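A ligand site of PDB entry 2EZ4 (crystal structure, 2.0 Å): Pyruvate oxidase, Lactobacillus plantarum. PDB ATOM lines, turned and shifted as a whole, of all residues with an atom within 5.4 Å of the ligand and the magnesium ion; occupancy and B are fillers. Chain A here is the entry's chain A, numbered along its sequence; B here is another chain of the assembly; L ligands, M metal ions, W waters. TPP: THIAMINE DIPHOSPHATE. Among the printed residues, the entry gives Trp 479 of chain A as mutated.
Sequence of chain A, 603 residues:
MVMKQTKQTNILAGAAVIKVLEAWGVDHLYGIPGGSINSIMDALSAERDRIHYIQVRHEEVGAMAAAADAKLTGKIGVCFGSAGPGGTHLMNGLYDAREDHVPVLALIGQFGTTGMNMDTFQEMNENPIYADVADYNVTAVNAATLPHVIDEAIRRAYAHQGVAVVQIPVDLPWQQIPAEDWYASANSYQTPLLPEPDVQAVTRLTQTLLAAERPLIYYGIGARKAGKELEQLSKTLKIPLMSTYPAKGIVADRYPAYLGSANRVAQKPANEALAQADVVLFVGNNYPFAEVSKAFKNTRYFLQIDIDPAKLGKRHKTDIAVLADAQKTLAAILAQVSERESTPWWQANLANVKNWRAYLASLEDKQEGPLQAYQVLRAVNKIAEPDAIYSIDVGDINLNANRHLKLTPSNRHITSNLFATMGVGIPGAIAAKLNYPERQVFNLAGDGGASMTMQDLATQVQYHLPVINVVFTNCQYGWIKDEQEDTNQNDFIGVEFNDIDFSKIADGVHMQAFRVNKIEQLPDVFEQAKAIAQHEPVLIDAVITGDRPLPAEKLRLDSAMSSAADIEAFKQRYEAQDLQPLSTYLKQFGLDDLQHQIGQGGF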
ATOM      1  N   ASN A  92       2.769  29.854 -31.720  1.00  0.00           N
ATOM      2  CA  ASN A  92       2.674  29.166 -30.428  1.00  0.00           C
ATOM      3  C   ASN A  92       3.834  29.457 -29.500  1.00  0.00           C
ATOM      4  O   ASN A  92       3.628  29.559 -28.281  1.00  0.00           O
ATOM      5  CB  ASN A  92       2.437  27.654 -30.565  1.00  0.00           C
ATOM      6  CG  ASN A  92       0.965  27.324 -30.827  1.00  0.00           C
ATOM      7  OD1 ASN A  92       0.348  27.889 -31.732  1.00  0.00           O
ATOM      8  ND2 ASN A  92       0.403  26.413 -30.048  1.00  0.00           N
ATOM      9  N   ASP A 393       7.059  18.907 -21.342  1.00  0.00           N
ATOM     10  CA  ASP A 393       5.952  19.214 -22.228  1.00  0.00           C
ATOM     11  C   ASP A 393       4.671  19.463 -21.396  1.00  0.00           C
ATOM     12  O   ASP A 393       4.752  19.823 -20.226  1.00  0.00           O
ATOM     13  CB  ASP A 393       5.761  18.104 -23.248  1.00  0.00           C
ATOM     14  CG  ASP A 393       5.295  18.608 -24.592  1.00  0.00           C
ATOM     15  OD1 ASP A 393       4.068  18.855 -24.748  1.00  0.00           O
ATOM     16  OD2 ASP A 393       6.142  18.724 -25.504  1.00  0.00           O
ATOM     17  N   VAL A 394       3.502  19.338 -22.026  1.00  0.00           N
ATOM     18  CA  VAL A 394       2.233  19.708 -21.394  1.00  0.00           C
ATOM     19  C   VAL A 394       1.280  18.517 -21.360  1.00  0.00           C
ATOM     20  O   VAL A 394       1.031  17.884 -22.382  1.00  0.00           O
ATOM     21  CB  VAL A 394       1.603  20.931 -22.144  1.00  0.00           C
ATOM     22  CG1 VAL A 394       0.172  21.193 -21.705  1.00  0.00           C
ATOM     23  CG2 VAL A 394       2.476  22.165 -21.929  1.00  0.00           C
ATOM     24  N   GLY A 395       0.706  18.244 -20.189  1.00  0.00           N
ATOM     25  CA  GLY A 395      -0.207  17.113 -20.014  1.00  0.00           C
ATOM     26  C   GLY A 395       0.048  16.440 -18.662  1.00  0.00           C
ATOM     27  O   GLY A 395       0.544  17.079 -17.747  1.00  0.00           O
ATOM     28  N   ASP A 396      -0.270  15.146 -18.556  1.00  0.00           N
ATOM     29  CA  ASP A 396      -0.011  14.387 -17.320  1.00  0.00           C
ATOM     30  C   ASP A 396       1.414  14.544 -16.809  1.00  0.00           C
ATOM     31  O   ASP A 396       1.626  14.500 -15.602  1.00  0.00           O
ATOM     32  CB  ASP A 396      -0.272  12.880 -17.502  1.00  0.00           C
ATOM     33  CG  ASP A 396      -1.718  12.498 -17.283  1.00  0.00           C
ATOM     34  OD1 ASP A 396      -2.547  13.342 -16.907  1.00  0.00           O
ATOM     35  OD2 ASP A 396      -2.034  11.298 -17.506  1.00  0.00           O
ATOM     36  N   ILE A 397       2.367  14.696 -17.716  1.00  0.00           N
ATOM     37  CA  ILE A 397       3.785  14.841 -17.350  1.00  0.00           C
ATOM     38  C   ILE A 397       4.056  16.013 -16.399  1.00  0.00           C
ATOM     39  O   ILE A 397       4.900  15.888 -15.519  1.00  0.00           O
ATOM     40  CB  ILE A 397       4.753  14.908 -18.597  1.00  0.00           C
ATOM     41  CG1 ILE A 397       6.228  14.797 -18.142  1.00  0.00           C
ATOM     42  CG2 ILE A 397       4.546  16.212 -19.428  1.00  0.00           C
ATOM     43  CD1 ILE A 397       6.616  13.472 -17.437  1.00  0.00           C
ATOM     44  N   PHE A 419       0.409  29.802 -21.108  1.00  0.00           N
ATOM     45  CA  PHE A 419      -0.159  29.484 -22.435  1.00  0.00           C
ATOM     46  C   PHE A 419      -0.281  27.978 -22.561  1.00  0.00           C
ATOM     47  O   PHE A 419      -1.212  27.475 -23.186  1.00  0.00           O
ATOM     48  CB  PHE A 419       0.741  30.025 -23.563  1.00  0.00           C
ATOM     49  CG  PHE A 419       0.077  30.053 -24.948  1.00  0.00           C
ATOM     50  CD1 PHE A 419      -1.122  30.754 -25.152  1.00  0.00           C
ATOM     51  CD2 PHE A 419       0.695  29.441 -26.038  1.00  0.00           C
ATOM     52  CE1 PHE A 419      -1.718  30.815 -26.448  1.00  0.00           C
ATOM     53  CE2 PHE A 419       0.120  29.478 -27.331  1.00  0.00           C
ATOM     54  CZ  PHE A 419      -1.105  30.189 -27.521  1.00  0.00           C
ATOM     55  N   ALA A 420       0.652  27.257 -21.941  1.00  0.00           N
ATOM     56  CA  ALA A 420       0.577  25.807 -21.855  1.00  0.00           C
ATOM     57  C   ALA A 420       0.425  25.161 -23.237  1.00  0.00           C
ATOM     58  O   ALA A 420      -0.454  24.305 -23.435  1.00  0.00           O
ATOM     59  CB  ALA A 420      -0.597  25.371 -20.909  1.00  0.00           C
ATOM     60  N   THR A 421       1.260  25.592 -24.187  1.00  0.00           N
ATOM     61  CA  THR A 421       1.332  24.937 -25.486  1.00  0.00           C
ATOM     62  C   THR A 421       2.051  23.600 -25.383  1.00  0.00           C
ATOM     63  O   THR A 421       3.191  23.526 -24.884  1.00  0.00           O
ATOM     64  CB  THR A 421       1.964  25.830 -26.594  1.00  0.00           C
ATOM     65  OG1 THR A 421       1.884  25.149 -27.848  1.00  0.00           O
ATOM     66  CG2 THR A 421       3.460  26.234 -26.298  1.00  0.00           C
ATOM     67  N   MET A 422       1.384  22.554 -25.856  1.00  0.00           N
ATOM     68  CA  MET A 422       2.005  21.258 -26.088  1.00  0.00           C
ATOM     69  C   MET A 422       3.086  21.412 -27.150  1.00  0.00           C
ATOM     70  O   MET A 422       3.061  22.365 -27.939  1.00  0.00           O
ATOM     71  CB  MET A 422       0.967  20.250 -26.581  1.00  0.00           C
ATOM     72  CG  MET A 422      -0.009  19.758 -25.522  1.00  0.00           C
ATOM     73  SD  MET A 422      -1.391  18.935 -26.335  1.00  0.00           S
ATOM     74  CE  MET A 422      -0.609  17.420 -26.899  1.00  0.00           C
ATOM     75  N   ALA A 445       8.067  14.270 -22.099  1.00  0.00           N
ATOM     76  CA  ALA A 445       6.902  14.620 -22.874  1.00  0.00           C
ATOM     77  C   ALA A 445       5.943  13.441 -23.023  1.00  0.00           C
ATOM     78  O   ALA A 445       6.377  12.283 -23.132  1.00  0.00           O
ATOM     79  CB  ALA A 445       7.335  15.123 -24.264  1.00  0.00           C
ATOM     80  N   GLY A 446       4.657  13.738 -23.031  1.00  0.00           N
ATOM     81  CA  GLY A 446       3.668  12.743 -23.428  1.00  0.00           C
ATOM     82  C   GLY A 446       3.724  12.514 -24.931  1.00  0.00           C
ATOM     83  O   GLY A 446       4.366  13.281 -25.669  1.00  0.00           O
ATOM     84  N   ASP A 447       3.061  11.445 -25.375  1.00  0.00           N
ATOM     85  CA  ASP A 447       3.016  11.098 -26.777  1.00  0.00           C
ATOM     86  C   ASP A 447       2.283  12.122 -27.637  1.00  0.00           C
ATOM     87  O   ASP A 447       2.680  12.378 -28.749  1.00  0.00           O
ATOM     88  CB  ASP A 447       2.493   9.670 -27.042  1.00  0.00           C
ATOM     89  CG  ASP A 447       1.188   9.328 -26.328  1.00  0.00           C
ATOM     90  OD1 ASP A 447       0.571  10.159 -25.622  1.00  0.00           O
ATOM     91  OD2 ASP A 447       0.777   8.157 -26.472  1.00  0.00           O
ATOM     92  N   GLY A 448       1.211  12.717 -27.108  1.00  0.00           N
ATOM     93  CA  GLY A 448       0.492  13.768 -27.825  1.00  0.00           C
ATOM     94  C   GLY A 448       1.379  14.960 -28.076  1.00  0.00           C
ATOM     95  O   GLY A 448       1.473  15.447 -29.198  1.00  0.00           O
ATOM     96  N   GLY A 449       2.042  15.463 -27.028  1.00  0.00           N
ATOM     97  CA  GLY A 449       2.911  16.648 -27.163  1.00  0.00           C
ATOM     98  C   GLY A 449       4.155  16.394 -27.991  1.00  0.00           C
ATOM     99  O   GLY A 449       4.528  17.197 -28.837  1.00  0.00           O
ATOM    100  N   ALA A 450       4.805  15.266 -27.744  1.00  0.00           N
ATOM    101  CA  ALA A 450       5.964  14.831 -28.540  1.00  0.00           C
ATOM    102  C   ALA A 450       5.642  14.677 -30.032  1.00  0.00           C
ATOM    103  O   ALA A 450       6.462  15.029 -30.887  1.00  0.00           O
ATOM    104  CB  ALA A 450       6.550  13.537 -27.959  1.00  0.00           C
ATOM    105  N   MET A 452       3.530  16.488 -31.732  1.00  0.00           N
ATOM    106  CA  MET A 452       3.373  17.799 -32.387  1.00  0.00           C
ATOM    107  C   MET A 452       4.671  18.404 -32.888  1.00  0.00           C
ATOM    108  O   MET A 452       4.661  19.130 -33.886  1.00  0.00           O
ATOM    109  CB  MET A 452       2.686  18.787 -31.439  1.00  0.00           C
ATOM    110  CG  MET A 452       1.205  18.470 -31.264  1.00  0.00           C
ATOM    111  SD  MET A 452       0.399  19.611 -30.156  1.00  0.00           S
ATOM    112  CE  MET A 452      -1.304  18.969 -30.243  1.00  0.00           C
ATOM    113  N   PHE A 472       6.293   9.476 -22.946  1.00  0.00           N
ATOM    114  CA  PHE A 472       5.320   8.726 -22.157  1.00  0.00           C
ATOM    115  C   PHE A 472       4.150   8.361 -23.042  1.00  0.00           C
ATOM    116  O   PHE A 472       3.255   9.175 -23.295  1.00  0.00           O
ATOM    117  CB  PHE A 472       4.860   9.549 -20.952  1.00  0.00           C
ATOM    118  CG  PHE A 472       5.957   9.794 -19.930  1.00  0.00           C
ATOM    119  CD1 PHE A 472       6.982  10.709 -20.196  1.00  0.00           C
ATOM    120  CD2 PHE A 472       5.976   9.088 -18.737  1.00  0.00           C
ATOM    121  CE1 PHE A 472       8.007  10.930 -19.263  1.00  0.00           C
ATOM    122  CE2 PHE A 472       6.993   9.326 -17.781  1.00  0.00           C
ATOM    123  CZ  PHE A 472       8.010  10.237 -18.051  1.00  0.00           C
ATOM    124  N   ASN A 474       0.961   6.627 -23.763  1.00  0.00           N
ATOM    125  CA  ASN A 474      -0.247   5.995 -23.249  1.00  0.00           C
ATOM    126  C   ASN A 474      -1.330   5.847 -24.316  1.00  0.00           C
ATOM    127  O   ASN A 474      -2.411   5.354 -24.021  1.00  0.00           O
ATOM    128  CB  ASN A 474      -0.779   6.740 -21.998  1.00  0.00           C
ATOM    129  CG  ASN A 474      -0.954   8.224 -22.219  1.00  0.00           C
ATOM    130  OD1 ASN A 474      -0.802   8.713 -23.335  1.00  0.00           O
ATOM    131  ND2 ASN A 474      -1.316   8.939 -21.171  1.00  0.00           N
ATOM    132  N   CYS A 475      -1.026   6.281 -25.547  1.00  0.00           N
ATOM    133  CA  CYS A 475      -1.988   6.277 -26.661  1.00  0.00           C
ATOM    134  C   CYS A 475      -3.247   7.079 -26.300  1.00  0.00           C
ATOM    135  O   CYS A 475      -4.361   6.732 -26.738  1.00  0.00           O
ATOM    136  CB  CYS A 475      -2.347   4.834 -27.068  1.00  0.00           C
ATOM    137  SG  CYS A 475      -0.919   3.912 -27.717  1.00  0.00           S
ATOM    138  N   GLN A 476      -3.049   8.136 -25.522  1.00  0.00           N
ATOM    139  CA  GLN A 476      -4.145   8.990 -25.077  1.00  0.00           C
ATOM    140  C   GLN A 476      -3.668  10.412 -24.976  1.00  0.00           C
ATOM    141  O   GLN A 476      -2.461  10.663 -24.877  1.00  0.00           O
ATOM    142  CB  GLN A 476      -4.646   8.576 -23.671  1.00  0.00           C
ATOM    143  CG  GLN A 476      -5.102   7.121 -23.542  1.00  0.00           C
ATOM    144  CD  GLN A 476      -5.448   6.730 -22.123  1.00  0.00           C
ATOM    145  OE1 GLN A 476      -6.172   5.763 -21.898  1.00  0.00           O
ATOM    146  NE2 GLN A 476      -4.931   7.482 -21.153  1.00  0.00           N
ATOM    147  N   TYR A 477      -4.610  11.339 -24.998  1.00  0.00           N
ATOM    148  CA  TYR A 477      -4.418  12.639 -24.404  1.00  0.00           C
ATOM    149  C   TYR A 477      -4.966  12.446 -23.002  1.00  0.00           C
ATOM    150  O   TYR A 477      -6.136  12.780 -22.736  1.00  0.00           O
ATOM    151  CB  TYR A 477      -5.238  13.726 -25.160  1.00  0.00           C
ATOM    152  CG  TYR A 477      -4.779  13.992 -26.585  1.00  0.00           C
ATOM    153  CD1 TYR A 477      -3.448  14.331 -26.872  1.00  0.00           C
ATOM    154  CD2 TYR A 477      -5.686  13.899 -27.653  1.00  0.00           C
ATOM    155  CE1 TYR A 477      -3.023  14.574 -28.205  1.00  0.00           C
ATOM    156  CE2 TYR A 477      -5.278  14.134 -28.973  1.00  0.00           C
ATOM    157  CZ  TYR A 477      -3.947  14.471 -29.238  1.00  0.00           C
ATOM    158  OH  TYR A 477      -3.559  14.695 -30.536  1.00  0.00           O
ATOM    159  N   GLY A 478      -4.140  11.884 -22.098  1.00  0.00           N
ATOM    160  CA  GLY A 478      -4.608  11.460 -20.783  1.00  0.00           C
ATOM    161  C   GLY A 478      -5.169  12.623 -19.974  1.00  0.00           C
ATOM    162  O   GLY A 478      -6.231  12.517 -19.384  1.00  0.00           O
ATOM    163  N   TRP A 479      -4.446  13.744 -19.969  1.00  0.00           N
ATOM    164  CA  TRP A 479      -4.882  14.973 -19.288  1.00  0.00           C
ATOM    165  C   TRP A 479      -6.334  15.312 -19.618  1.00  0.00           C
ATOM    166  O   TRP A 479      -7.116  15.684 -18.715  1.00  0.00           O
ATOM    167  CB  TRP A 479      -3.958  16.128 -19.681  1.00  0.00           C
ATOM    168  CG  TRP A 479      -4.008  17.363 -18.786  1.00  0.00           C
ATOM    169  CD1 TRP A 479      -4.509  18.594 -19.103  1.00  0.00           C
ATOM    170  CD2 TRP A 479      -3.492  17.471 -17.444  1.00  0.00           C
ATOM    171  NE1 TRP A 479      -4.350  19.468 -18.041  1.00  0.00           N
ATOM    172  CE2 TRP A 479      -3.719  18.800 -17.011  1.00  0.00           C
ATOM    173  CE3 TRP A 479      -2.867  16.573 -16.566  1.00  0.00           C
ATOM    174  CZ2 TRP A 479      -3.345  19.257 -15.738  1.00  0.00           C
ATOM    175  CZ3 TRP A 479      -2.485  17.033 -15.288  1.00  0.00           C
ATOM    176  CH2 TRP A 479      -2.736  18.367 -14.899  1.00  0.00           C
ATOM    177  N   ILE A 480      -6.696  15.190 -20.901  1.00  0.00           N
ATOM    178  CA  ILE A 480      -8.040  15.545 -21.381  1.00  0.00           C
ATOM    179  C   ILE A 480      -9.055  14.413 -21.198  1.00  0.00           C
ATOM    180  O   ILE A 480     -10.239  14.665 -20.940  1.00  0.00           O
ATOM    181  CB  ILE A 480      -8.019  15.978 -22.877  1.00  0.00           C
ATOM    182  CG1 ILE A 480      -6.898  17.009 -23.131  1.00  0.00           C
ATOM    183  CG2 ILE A 480      -9.414  16.517 -23.328  1.00  0.00           C
ATOM    184  CD1 ILE A 480      -6.941  18.202 -22.222  1.00  0.00           C
ATOM    185  N   PHE A 497      -6.176   7.209 -28.965  1.00  0.00           N
ATOM    186  CA  PHE A 497      -5.759   7.137 -30.349  1.00  0.00           C
ATOM    187  C   PHE A 497      -4.735   6.039 -30.602  1.00  0.00           C
ATOM    188  O   PHE A 497      -4.307   5.336 -29.682  1.00  0.00           O
ATOM    189  CB  PHE A 497      -5.239   8.506 -30.818  1.00  0.00           C
ATOM    190  CG  PHE A 497      -4.221   9.140 -29.892  1.00  0.00           C
ATOM    191  CD1 PHE A 497      -2.931   8.616 -29.765  1.00  0.00           C
ATOM    192  CD2 PHE A 497      -4.560  10.285 -29.154  1.00  0.00           C
ATOM    193  CE1 PHE A 497      -1.986   9.215 -28.920  1.00  0.00           C
ATOM    194  CE2 PHE A 497      -3.619  10.893 -28.308  1.00  0.00           C
ATOM    195  CZ  PHE A 497      -2.350  10.361 -28.182  1.00  0.00           C
ATOM    196  N   ILE B  32      -8.543  18.802 -32.080  1.00  0.00           N
ATOM    197  CA  ILE B  32      -7.975  18.150 -30.914  1.00  0.00           C
ATOM    198  C   ILE B  32      -8.738  18.712 -29.715  1.00  0.00           C
ATOM    199  O   ILE B  32      -8.929  19.944 -29.627  1.00  0.00           O
ATOM    200  CB  ILE B  32      -6.442  18.441 -30.772  1.00  0.00           C
ATOM    201  CG1 ILE B  32      -5.685  17.820 -31.946  1.00  0.00           C
ATOM    202  CG2 ILE B  32      -5.907  17.984 -29.369  1.00  0.00           C
ATOM    203  CD1 ILE B  32      -4.182  18.056 -31.961  1.00  0.00           C
ATOM    204  N   PRO B  33      -9.215  17.828 -28.828  1.00  0.00           N
ATOM    205  CA  PRO B  33     -10.048  18.268 -27.699  1.00  0.00           C
ATOM    206  C   PRO B  33      -9.198  18.949 -26.645  1.00  0.00           C
ATOM    207  O   PRO B  33      -7.973  18.871 -26.694  1.00  0.00           O
ATOM    208  CB  PRO B  33     -10.629  16.963 -27.148  1.00  0.00           C
ATOM    209  CG  PRO B  33      -9.582  15.927 -27.498  1.00  0.00           C
ATOM    210  CD  PRO B  33      -9.012  16.353 -28.821  1.00  0.00           C
ATOM    211  N   GLY B  34      -9.869  19.628 -25.712  1.00  0.00           N
ATOM    212  CA  GLY B  34      -9.209  20.230 -24.556  1.00  0.00           C
ATOM    213  C   GLY B  34     -10.315  20.587 -23.596  1.00  0.00           C
ATOM    214  O   GLY B  34     -11.485  20.651 -23.997  1.00  0.00           O
ATOM    215  N   GLU B  59      -3.152  20.642 -34.606  1.00  0.00           N
ATOM    216  CA  GLU B  59      -4.323  21.419 -35.050  1.00  0.00           C
ATOM    217  C   GLU B  59      -4.169  22.104 -36.395  1.00  0.00           C
ATOM    218  O   GLU B  59      -5.178  22.368 -37.050  1.00  0.00           O
ATOM    219  CB  GLU B  59      -4.807  22.420 -33.999  1.00  0.00           C
ATOM    220  CG  GLU B  59      -5.266  21.783 -32.708  1.00  0.00           C
ATOM    221  CD  GLU B  59      -4.138  21.626 -31.687  1.00  0.00           C
ATOM    222  OE1 GLU B  59      -2.940  21.697 -32.072  1.00  0.00           O
ATOM    223  OE2 GLU B  59      -4.446  21.433 -30.478  1.00  0.00           O
ATOM    224  N   SER B  82      -8.676  23.977 -29.114  1.00  0.00           N
ATOM    225  CA  SER B  82      -8.908  24.403 -27.730  1.00  0.00           C
ATOM    226  C   SER B  82      -8.316  25.804 -27.441  1.00  0.00           C
ATOM    227  O   SER B  82      -7.538  26.352 -28.246  1.00  0.00           O
ATOM    228  CB  SER B  82      -8.335  23.365 -26.758  1.00  0.00           C
ATOM    229  OG  SER B  82      -6.971  23.141 -27.069  1.00  0.00           O
ATOM    230  N   PRO B  85      -3.272  27.739 -27.220  1.00  0.00           N
ATOM    231  CA  PRO B  85      -2.428  27.073 -28.203  1.00  0.00           C
ATOM    232  C   PRO B  85      -3.135  26.165 -29.208  1.00  0.00           C
ATOM    233  O   PRO B  85      -2.606  25.952 -30.303  1.00  0.00           O
ATOM    234  CB  PRO B  85      -1.463  26.248 -27.345  1.00  0.00           C
ATOM    235  CG  PRO B  85      -2.164  26.052 -26.052  1.00  0.00           C
ATOM    236  CD  PRO B  85      -2.957  27.308 -25.835  1.00  0.00           C
ATOM    237  N   GLY B  86      -4.295  25.622 -28.852  1.00  0.00           N
ATOM    238  CA  GLY B  86      -5.063  24.790 -29.783  1.00  0.00           C
ATOM    239  C   GLY B  86      -5.497  25.644 -30.973  1.00  0.00           C
ATOM    240  O   GLY B  86      -5.263  25.297 -32.125  1.00  0.00           O
ATOM    241  N   HIS B  89      -2.601  27.162 -33.165  1.00  0.00           N
ATOM    242  CA  HIS B  89      -2.053  26.144 -34.086  1.00  0.00           C
ATOM    243  C   HIS B  89      -2.812  26.094 -35.426  1.00  0.00           C
ATOM    244  O   HIS B  89      -2.275  25.638 -36.440  1.00  0.00           O
ATOM    245  CB  HIS B  89      -2.061  24.751 -33.432  1.00  0.00           C
ATOM    246  CG  HIS B  89      -0.752  24.338 -32.837  1.00  0.00           C
ATOM    247  ND1 HIS B  89      -0.594  23.165 -32.129  1.00  0.00           N
ATOM    248  CD2 HIS B  89       0.474  24.915 -32.874  1.00  0.00           C
ATOM    249  CE1 HIS B  89       0.665  23.054 -31.745  1.00  0.00           C
ATOM    250  NE2 HIS B  89       1.335  24.102 -32.178  1.00  0.00           N
ATOM    251  N   GLN B 122      -4.472  29.482 -19.068  1.00  0.00           N
ATOM    252  CA  GLN B 122      -4.679  29.440 -20.517  1.00  0.00           C
ATOM    253  C   GLN B 122      -5.836  30.334 -20.976  1.00  0.00           C
ATOM    254  O   GLN B 122      -6.481  30.067 -22.002  1.00  0.00           O
ATOM    255  CB  GLN B 122      -4.924  27.992 -20.927  1.00  0.00           C
ATOM    256  CG  GLN B 122      -4.358  27.595 -22.231  1.00  0.00           C
ATOM    257  CD  GLN B 122      -4.414  26.112 -22.422  1.00  0.00           C
ATOM    258  OE1 GLN B 122      -5.411  25.467 -22.109  1.00  0.00           O
ATOM    259  NE2 GLN B 122      -3.334  25.541 -22.940  1.00  0.00           N
HETATM  260  N1' TPP L   1      -3.319  21.714 -28.200  1.00  0.00           N
HETATM  261  C2' TPP L   1      -2.174  22.409 -27.851  1.00  0.00           C
HETATM  262  CM2 TPP L   1      -1.202  22.886 -28.894  1.00  0.00           C
HETATM  263  N3' TPP L   1      -1.864  22.670 -26.529  1.00  0.00           N
HETATM  264  C4' TPP L   1      -2.708  22.262 -25.518  1.00  0.00           C
HETATM  265  N4' TPP L   1      -2.380  22.581 -24.263  1.00  0.00           N
HETATM  266  C5' TPP L   1      -3.878  21.566 -25.845  1.00  0.00           C
HETATM  267  C6' TPP L   1      -4.179  21.288 -27.191  1.00  0.00           C
HETATM  268  C7' TPP L   1      -4.805  21.070 -24.741  1.00  0.00           C
HETATM  269  N3  TPP L   1      -4.165  19.953 -24.035  1.00  0.00           N
HETATM  270  C2  TPP L   1      -3.514  20.030 -22.797  1.00  0.00           C
HETATM  271  S1  TPP L   1      -2.872  18.632 -22.243  1.00  0.00           S
HETATM  272  C5  TPP L   1      -3.414  17.855 -23.566  1.00  0.00           C
HETATM  273  C4  TPP L   1      -4.105  18.662 -24.480  1.00  0.00           C
HETATM  274  CM4 TPP L   1      -4.684  18.128 -25.773  1.00  0.00           C
HETATM  275  C6  TPP L   1      -3.140  16.364 -23.667  1.00  0.00           C
HETATM  276  C7  TPP L   1      -1.659  16.010 -23.661  1.00  0.00           C
HETATM  277  O7  TPP L   1      -1.529  14.677 -24.154  1.00  0.00           O
HETATM  278  PA  TPP L   1      -0.133  13.935 -24.005  1.00  0.00           P
HETATM  279  O1A TPP L   1      -0.193  12.590 -24.687  1.00  0.00           O
HETATM  280  O2A TPP L   1       0.976  14.805 -24.485  1.00  0.00           O
HETATM  281  O3A TPP L   1       0.073  13.756 -22.416  1.00  0.00           O
HETATM  282  PB  TPP L   1      -0.678  12.712 -21.422  1.00  0.00           P
HETATM  283  O1B TPP L   1      -1.665  13.491 -20.578  1.00  0.00           O
HETATM  284  O2B TPP L   1       0.463  12.175 -20.610  1.00  0.00           O
HETATM  285  O3B TPP L   1      -1.366  11.606 -22.188  1.00  0.00           O
HETATM  286 MG    MG M   1      -0.494  10.781 -23.977  1.00  0.00          MG
HETATM  287  O   HOH W   1      -5.682  24.473 -25.137  1.00  0.00           O
HETATM  288  O   HOH W   2      -4.306  23.054 -21.906  1.00  0.00           O
HETATM  289  O   HOH W   3       1.792  10.329 -19.014  1.00  0.00           O
HETATM  290  O   HOH W   4       2.323  14.257 -20.595  1.00  0.00           O
HETATM  291  O   HOH W   5       2.696  15.911 -22.963  1.00  0.00           O
HETATM  292  O   HOH W   6       1.305  10.736 -22.653  1.00  0.00           O
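A nitrogen (N1') of the ligand lies within hydrogen-bond range of the side-chain carboxylate (OE2) of Glu 59 of chain B (2.6 Å). The backbone carbonyl oxygen (O) of Ala 420 lies within hydrogen-bond range of a nitrogen (N4') of the ligand (2.7 Å). The backbone NH (N) of Gly 478 is in hydrogen-bond range of an oxygen (O1B) of the ligand (3.3 Å). The backbone NH of Gly 448 lies within hydrogen-bond range of an oxygen (O2A) of the ligand (3.4 Å). The backbone NH (N) of Gly 449 sits at hydrogen-bond distance from an oxygen (O2A) of the ligand (2.8 Å). The backbone NH (N) of Trp 479 lies within hydrogen-bond range of an oxygen (O1B) of the ligand, at 2.9 Å. N of Asp 396 lies within hydrogen-bond range of O1B of the ligand (3.0 Å). N of Met 422 sits at hydrogen-bond distance from N3' of the ligand, 3.3 Å away. The side-chain amide nitrogen of Gln 122 of chain B sits close to a nitrogen (N4') of the ligand, 3.4 Å away.
The backbone NH (N) of Asp 447 sits at hydrogen-bond distance from the backbone carbonyl oxygen (O) of Phe 472 (3.1 Å). The side-chain carboxylate (OD2) of Asp 447 sits at hydrogen-bond distance from the backbone NH (N) of Cys 475, at 2.8 Å. OE1 of Glu 59 of chain B is in hydrogen-bond range of ND1 of His 89 of chain B (2.8 Å). The backbone carbonyl oxygen of Ala 420 lies within hydrogen-bond range of the side-chain amide nitrogen of Gln 122 of chain B (3.2 Å). A ring nitrogen (NE2) of His 89 of chain B lies close to the side-chain amide nitrogen of Asn 92, at 3.3 Å. The side-chain amide nitrogen (NE2) of Gln 122 of chain B lies within hydrogen-bond range of the backbone carbonyl oxygen (O) of Phe 419, at 2.9 Å. ND2 of Asn 92 lies within hydrogen-bond range of O of Pro 85 of chain B, 3.1 Å away. ND2 of Asn 92 sits at hydrogen-bond distance from OG1 of Thr 421, at 2.9 Å.
Val 394 touches the ligand (O to C7, 3.5 Å). CA of Gly 395 touches S1 of the ligand (3.8 Å). Thr 421 touches the ligand. Gly 446 touches the ligand. Met 452 touches the ligand. Tyr 477 touches the ligand (CD1 to O7, 3.3 Å). Ile 480 touches the ligand. Ile 32 of chain B touches the ligand (CG2 to CM4, 3.8 Å). O of Pro 33 of chain B touches CM4 of the ligand, 3.5 Å away. Ser 82 of chain B touches the ligand (OG to C6', 3.4 Å). CG of Pro 85 of chain B touches N3' of the ligand, at 3.4 Å. Gly 86 of chain B touches the ligand (CA to N1', 3.9 Å). ND1 of His 89 of chain B touches CM2 of the ligand (3.3 Å). Hydrophobic or aromatic side chains that line the ligand: Val 394, Met 422, Met 452, Tyr 477, Trp 479, Ile 480, Ile 32 of chain B, Pro 85 of chain B and His 89 of chain B. 25 residues have an atom within 4 Å of the ligand: Val 394, Gly 395, Asp 396, Ala 420, Thr 421, Met 422, Gly 446, Asp 447, Gly 448, Gly 449, Met 452, Asn 474, Gln 476, Tyr 477, Gly 478, Trp 479, Ile 480, Ile 32 of chain B, Pro 33 of chain B, Glu 59 of chain B, Ser 82 of chain B, Pro 85 of chain B, Gly 86 of chain B, His 89 of chain B and Gln 122 of chain B. The nearest printed residue that does not touch the ligand is Asn 92 (4.04 Å).
Three residues have an atom within 4 Å of the magnesium ion: Asp 447, Asn 474 and Gln 476.
The magnesium ion is bound by an oxygen (O1A) of the ligand (2.0 Å), the side-chain carboxylate (OD1) of Asp 447 (2.1 Å), an oxygen (O3B) of the ligand (2.2 Å), the backbone carbonyl oxygen (O) of Gln 476 (2.2 Å), the side-chain amide oxygen (OD1) of Asn 474 (2.2 Å) and water W6 (2.2 Å). The magnesium ion has six donor atoms within binding distance.
Water W6 lies within hydrogen-bond range of O of Phe 472 (2.6 Å), O2B of the ligand (2.6 Å) and N of Asp 447 (3.3 Å). Water W5 lies within hydrogen-bond range of an oxygen (O2A) of the ligand, the backbone carbonyl oxygen (O) of Val 394 and the backbone NH (N) of Gly 446. Water W2 bridges OE1 of Gln 122 of chain B and N4' of the ligand. Water W1 bridges OG of Ser 82 of chain B (2.7 Å) and OE1 of Gln 122 of chain B (3.2 Å).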
